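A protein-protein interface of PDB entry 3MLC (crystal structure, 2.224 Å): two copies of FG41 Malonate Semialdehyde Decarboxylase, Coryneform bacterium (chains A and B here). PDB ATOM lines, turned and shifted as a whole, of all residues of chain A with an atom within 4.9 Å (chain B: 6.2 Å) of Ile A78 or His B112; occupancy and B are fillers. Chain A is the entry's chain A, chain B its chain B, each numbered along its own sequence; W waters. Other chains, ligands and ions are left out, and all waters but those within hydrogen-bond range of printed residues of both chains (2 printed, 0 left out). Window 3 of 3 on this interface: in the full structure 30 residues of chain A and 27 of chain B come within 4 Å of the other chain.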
ATOM      1  N   ARG A  76      31.878  14.611  34.935  1.00  0.00           N
ATOM      2  CA  ARG A  76      30.565  14.044  34.678  1.00  0.00           C
ATOM      3  C   ARG A  76      30.416  13.519  33.266  1.00  0.00           C
ATOM      4  O   ARG A  76      30.914  14.092  32.283  1.00  0.00           O
ATOM      5  CB  ARG A  76      29.439  15.050  34.975  1.00  0.00           C
ATOM      6  CG  ARG A  76      28.806  14.939  36.375  1.00  0.00           C
ATOM      7  CD  ARG A  76      29.802  15.149  37.506  1.00  0.00           C
ATOM      8  NE  ARG A  76      29.137  15.382  38.790  1.00  0.00           N
ATOM      9  CZ  ARG A  76      29.150  14.539  39.823  1.00  0.00           C
ATOM     10  NH1 ARG A  76      29.795  13.371  39.750  1.00  0.00           N
ATOM     11  NH2 ARG A  76      28.516  14.870  40.943  1.00  0.00           N
ATOM     12  N   THR A  77      29.683  12.424  33.202  1.00  0.00           N
ATOM     13  CA  THR A  77      29.441  11.658  31.997  1.00  0.00           C
ATOM     14  C   THR A  77      28.383  12.346  31.113  1.00  0.00           C
ATOM     15  O   THR A  77      27.582  13.140  31.621  1.00  0.00           O
ATOM     16  CB  THR A  77      28.999  10.242  32.451  1.00  0.00           C
ATOM     17  OG1 THR A  77      30.123   9.351  32.384  1.00  0.00           O
ATOM     18  CG2 THR A  77      27.908   9.732  31.618  1.00  0.00           C
ATOM     19  N   ILE A  78      28.390  12.033  29.810  1.00  0.00           N
ATOM     20  CA  ILE A  78      27.387  12.527  28.840  1.00  0.00           C
ATOM     21  C   ILE A  78      25.953  12.222  29.279  1.00  0.00           C
ATOM     22  O   ILE A  78      25.054  13.080  29.155  1.00  0.00           O
ATOM     23  CB  ILE A  78      27.644  11.980  27.376  1.00  0.00           C
ATOM     24  CG1 ILE A  78      28.951  12.560  26.801  1.00  0.00           C
ATOM     25  CG2 ILE A  78      26.455  12.259  26.436  1.00  0.00           C
ATOM     26  CD1 ILE A  78      29.560  11.785  25.633  1.00  0.00           C
ATOM     27  N   GLU A  79      25.752  11.014  29.815  1.00  0.00           N
ATOM     28  CA  GLU A  79      24.433  10.546  30.284  1.00  0.00           C
ATOM     29  C   GLU A  79      24.010  11.157  31.626  1.00  0.00           C
ATOM     30  O   GLU A  79      22.830  11.456  31.826  1.00  0.00           O
ATOM     31  CB  GLU A  79      24.405   9.009  30.364  1.00  0.00           C
ATOM     32  CG  GLU A  79      24.515   8.312  29.016  1.00  0.00           C
ATOM     33  CD  GLU A  79      25.925   8.203  28.492  1.00  0.00           C
ATOM     34  OE1 GLU A  79      26.055   8.007  27.261  1.00  0.00           O
ATOM     35  OE2 GLU A  79      26.896   8.312  29.291  1.00  0.00           O
ATOM     36  N   THR A  80      24.969  11.329  32.537  1.00  0.00           N
ATOM     37  CA  THR A  80      24.767  12.117  33.770  1.00  0.00           C
ATOM     38  C   THR A  80      24.261  13.534  33.427  1.00  0.00           C
ATOM     39  O   THR A  80      23.234  13.996  33.962  1.00  0.00           O
ATOM     40  CB  THR A  80      26.066  12.197  34.634  1.00  0.00           C
ATOM     41  OG1 THR A  80      26.522  10.875  34.951  1.00  0.00           O
ATOM     42  CG2 THR A  80      25.826  12.957  35.944  1.00  0.00           C
ATOM     43  N   LYS A  81      24.952  14.200  32.503  1.00  0.00           N
ATOM     44  CA  LYS A  81      24.516  15.505  32.002  1.00  0.00           C
ATOM     45  C   LYS A  81      23.122  15.460  31.370  1.00  0.00           C
ATOM     46  O   LYS A  81      22.293  16.330  31.639  1.00  0.00           O
ATOM     47  CB  LYS A  81      25.539  16.086  31.037  1.00  0.00           C
ATOM     48  CG  LYS A  81      26.881  16.276  31.652  1.00  0.00           C
ATOM     49  CD  LYS A  81      27.784  17.063  30.735  1.00  0.00           C
ATOM     50  CE  LYS A  81      29.157  17.172  31.326  1.00  0.00           C
ATOM     51  NZ  LYS A  81      30.182  17.254  30.263  1.00  0.00           N
ATOM     52  N   GLN A  82      22.863  14.456  30.531  1.00  0.00           N
ATOM     53  CA  GLN A  82      21.504  14.212  29.994  1.00  0.00           C
ATOM     54  C   GLN A  82      20.450  14.016  31.094  1.00  0.00           C
ATOM     55  O   GLN A  82      19.316  14.504  30.980  1.00  0.00           O
ATOM     56  CB  GLN A  82      21.485  12.986  29.073  1.00  0.00           C
ATOM     57  CG  GLN A  82      22.203  13.152  27.762  1.00  0.00           C
ATOM     58  CD  GLN A  82      21.973  11.972  26.842  1.00  0.00           C
ATOM     59  OE1 GLN A  82      22.775  11.020  26.796  1.00  0.00           O
ATOM     60  NE2 GLN A  82      20.864  12.014  26.109  1.00  0.00           N
ATOM     61  N   PHE A  85      19.818  17.507  32.636  1.00  0.00           N
ATOM     62  CA  PHE A  85      18.904  18.319  31.803  1.00  0.00           C
ATOM     63  C   PHE A  85      17.441  17.921  32.009  1.00  0.00           C
ATOM     64  O   PHE A  85      16.540  18.779  32.060  1.00  0.00           O
ATOM     65  CB  PHE A  85      19.248  18.216  30.310  1.00  0.00           C
ATOM     66  CG  PHE A  85      20.653  18.659  29.939  1.00  0.00           C
ATOM     67  CD1 PHE A  85      21.275  19.759  30.570  1.00  0.00           C
ATOM     68  CD2 PHE A  85      21.341  17.999  28.914  1.00  0.00           C
ATOM     69  CE1 PHE A  85      22.562  20.157  30.214  1.00  0.00           C
ATOM     70  CE2 PHE A  85      22.653  18.409  28.541  1.00  0.00           C
ATOM     71  CZ  PHE A  85      23.257  19.490  29.200  1.00  0.00           C
ATOM     72  N   ALA B 110      31.540  21.337  25.318  1.00  0.00           N
ATOM     73  CA  ALA B 110      31.174  20.323  24.323  1.00  0.00           C
ATOM     74  C   ALA B 110      29.693  20.444  23.905  1.00  0.00           C
ATOM     75  O   ALA B 110      28.915  21.117  24.573  1.00  0.00           O
ATOM     76  CB  ALA B 110      31.478  18.923  24.835  1.00  0.00           C
ATOM     77  N   PRO B 111      29.330  19.849  22.753  1.00  0.00           N
ATOM     78  CA  PRO B 111      27.932  19.727  22.301  1.00  0.00           C
ATOM     79  C   PRO B 111      27.019  18.973  23.285  1.00  0.00           C
ATOM     80  O   PRO B 111      25.811  19.230  23.342  1.00  0.00           O
ATOM     81  CB  PRO B 111      28.052  18.966  20.984  1.00  0.00           C
ATOM     82  CG  PRO B 111      29.479  19.168  20.527  1.00  0.00           C
ATOM     83  CD  PRO B 111      30.303  19.347  21.749  1.00  0.00           C
ATOM     84  N   HIS B 112      27.591  18.051  24.048  1.00  0.00           N
ATOM     85  CA  HIS B 112      26.841  17.391  25.100  1.00  0.00           C
ATOM     86  C   HIS B 112      26.542  18.302  26.324  1.00  0.00           C
ATOM     87  O   HIS B 112      25.908  17.869  27.295  1.00  0.00           O
ATOM     88  CB  HIS B 112      27.493  16.050  25.483  1.00  0.00           C
ATOM     89  CG  HIS B 112      28.946  16.134  25.834  1.00  0.00           C
ATOM     90  ND1 HIS B 112      29.397  16.761  26.977  1.00  0.00           N
ATOM     91  CD2 HIS B 112      30.040  15.611  25.234  1.00  0.00           C
ATOM     92  CE1 HIS B 112      30.712  16.646  27.053  1.00  0.00           C
ATOM     93  NE2 HIS B 112      31.127  15.949  26.008  1.00  0.00           N
ATOM     94  N   ASP B 113      26.978  19.571  26.253  1.00  0.00           N
ATOM     95  CA  ASP B 113      26.820  20.509  27.369  1.00  0.00           C
ATOM     96  C   ASP B 113      25.669  21.483  27.160  1.00  0.00           C
ATOM     97  O   ASP B 113      25.608  22.508  27.824  1.00  0.00           O
ATOM     98  CB  ASP B 113      28.118  21.286  27.597  1.00  0.00           C
ATOM     99  CG  ASP B 113      29.231  20.414  28.142  1.00  0.00           C
ATOM    100  OD1 ASP B 113      30.417  20.641  27.791  1.00  0.00           O
ATOM    101  OD2 ASP B 113      28.919  19.499  28.928  1.00  0.00           O
ATOM    102  N   TRP B 114      24.747  21.136  26.270  1.00  0.00           N
ATOM    103  CA  TRP B 114      23.716  22.065  25.778  1.00  0.00           C
ATOM    104  C   TRP B 114      22.314  21.442  25.785  1.00  0.00           C
ATOM    105  O   TRP B 114      22.131  20.366  25.249  1.00  0.00           O
ATOM    106  CB  TRP B 114      24.096  22.519  24.347  1.00  0.00           C
ATOM    107  CG  TRP B 114      25.338  23.416  24.280  1.00  0.00           C
ATOM    108  CD1 TRP B 114      26.626  23.044  23.958  1.00  0.00           C
ATOM    109  CD2 TRP B 114      25.390  24.816  24.572  1.00  0.00           C
ATOM    110  NE1 TRP B 114      27.463  24.124  24.033  1.00  0.00           N
ATOM    111  CE2 TRP B 114      26.728  25.230  24.394  1.00  0.00           C
ATOM    112  CE3 TRP B 114      24.428  25.769  24.943  1.00  0.00           C
ATOM    113  CZ2 TRP B 114      27.131  26.556  24.590  1.00  0.00           C
ATOM    114  CZ3 TRP B 114      24.836  27.083  25.152  1.00  0.00           C
ATOM    115  CH2 TRP B 114      26.178  27.460  24.975  1.00  0.00           C
ATOM    116  N   ALA B 121      19.233  17.024  25.307  1.00  0.00           N
ATOM    117  CA  ALA B 121      20.489  17.474  24.728  1.00  0.00           C
ATOM    118  C   ALA B 121      20.469  17.210  23.206  1.00  0.00           C
ATOM    119  O   ALA B 121      20.861  16.132  22.739  1.00  0.00           O
ATOM    120  CB  ALA B 121      21.649  16.762  25.415  1.00  0.00           C
ATOM    121  N   TYR B 123      22.058  17.941  20.607  1.00  0.00           N
ATOM    122  CA  TYR B 123      23.270  17.524  19.902  1.00  0.00           C
ATOM    123  C   TYR B 123      23.577  16.040  20.176  1.00  0.00           C
ATOM    124  O   TYR B 123      24.158  15.349  19.317  1.00  0.00           O
ATOM    125  CB  TYR B 123      24.471  18.381  20.305  1.00  0.00           C
ATOM    126  CG  TYR B 123      24.442  19.854  19.893  1.00  0.00           C
ATOM    127  CD1 TYR B 123      24.348  20.230  18.547  1.00  0.00           C
ATOM    128  CD2 TYR B 123      24.572  20.865  20.855  1.00  0.00           C
ATOM    129  CE1 TYR B 123      24.339  21.595  18.167  1.00  0.00           C
ATOM    130  CE2 TYR B 123      24.572  22.222  20.492  1.00  0.00           C
ATOM    131  CZ  TYR B 123      24.459  22.581  19.145  1.00  0.00           C
ATOM    132  OH  TYR B 123      24.471  23.921  18.787  1.00  0.00           O
ATOM    133  N   VAL B 124      23.209  15.578  21.376  1.00  0.00           N
ATOM    134  CA  VAL B 124      23.350  14.178  21.761  1.00  0.00           C
ATOM    135  C   VAL B 124      22.270  13.309  21.084  1.00  0.00           C
ATOM    136  O   VAL B 124      22.583  12.272  20.516  1.00  0.00           O
ATOM    137  CB  VAL B 124      23.338  13.976  23.307  1.00  0.00           C
ATOM    138  CG1 VAL B 124      23.464  12.487  23.664  1.00  0.00           C
ATOM    139  CG2 VAL B 124      24.475  14.762  23.974  1.00  0.00           C
HETATM  140  O   HOH W   1      24.813  15.126  27.492  1.00  0.00           O
HETATM  141  O   HOH W   2      18.988  14.132  26.090  1.00  0.00           O
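N of Ala B110 is in hydrogen-bond range of OD1 of Asp B113 (2.8 Å).
O of Ala B110 sits close to NE1 of Trp B114 (3.4 Å).
A ring nitrogen (ND1) of His B112 sits at hydrogen-bond distance from the side-chain carboxylate of Asp B113 (3.4 Å).
ND1 of His B112 sits close to NZ of Lys A81 (3.4 Å).
The side-chain amino group (NZ) of Lys A81 is in salt-bridge range of the side-chain carboxylate (OD2) of Asp B113 (2.9 Å).
Hydrophobic or aromatic side chains of chain A within 4 Å of the printed part of chain B: Ile A78 and Phe A85.
Along chain A the printed residues that touch a printed residue of chain B span positions 78 to 85.
Hydrophobic or aromatic side chains of chain B that line the printed part of chain A: His B112, Ala B121 and Val B124.
Among the printed residues, 8 pairs touch across the chains.
Among the printed residues, Asp or Glu carboxylates within 4 Å of a Lys or Arg side-chain nitrogen of the other chain: Lys A81 with Asp B113 (2.9 Å).
No position is printed for both chains.
Among the printed residues, pairs that only touch across the chains: Ile A78 with His B112 (3.6 Å), Gln A82 with Val B124 (3.5 Å), Phe A85 with His B112 (3.5 Å), Phe A85 with Asp B113 (3.7 Å), Phe A85 with Trp B114 (3.7 Å) and Phe A85 with Ala B121 (3.7 Å).
Of chain B, only His B112 (3.6 Å) comes within 4 Å of Ile A78.
Printed residues of chain A within 4 Å of His B112: Ile A78, Lys A81 and Phe A85.
Of the printed residues of chain A, Trp B114 touches Phe A85 (3.7 Å).
Printed residues of chain A within 4 Å of Ala B121: Phe A85 (3.7 Å).
The nearest residue of chain B that does not touch Ile A78 is Val B124 (4.03 Å).
Water W1 bridges the backbone carbonyl oxygen (O) of Ile A78 and the backbone carbonyl oxygen (O) of His B112.
Water W2 lies within hydrogen-bond range of NE2 of Gln A82 and N of Ala B121.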
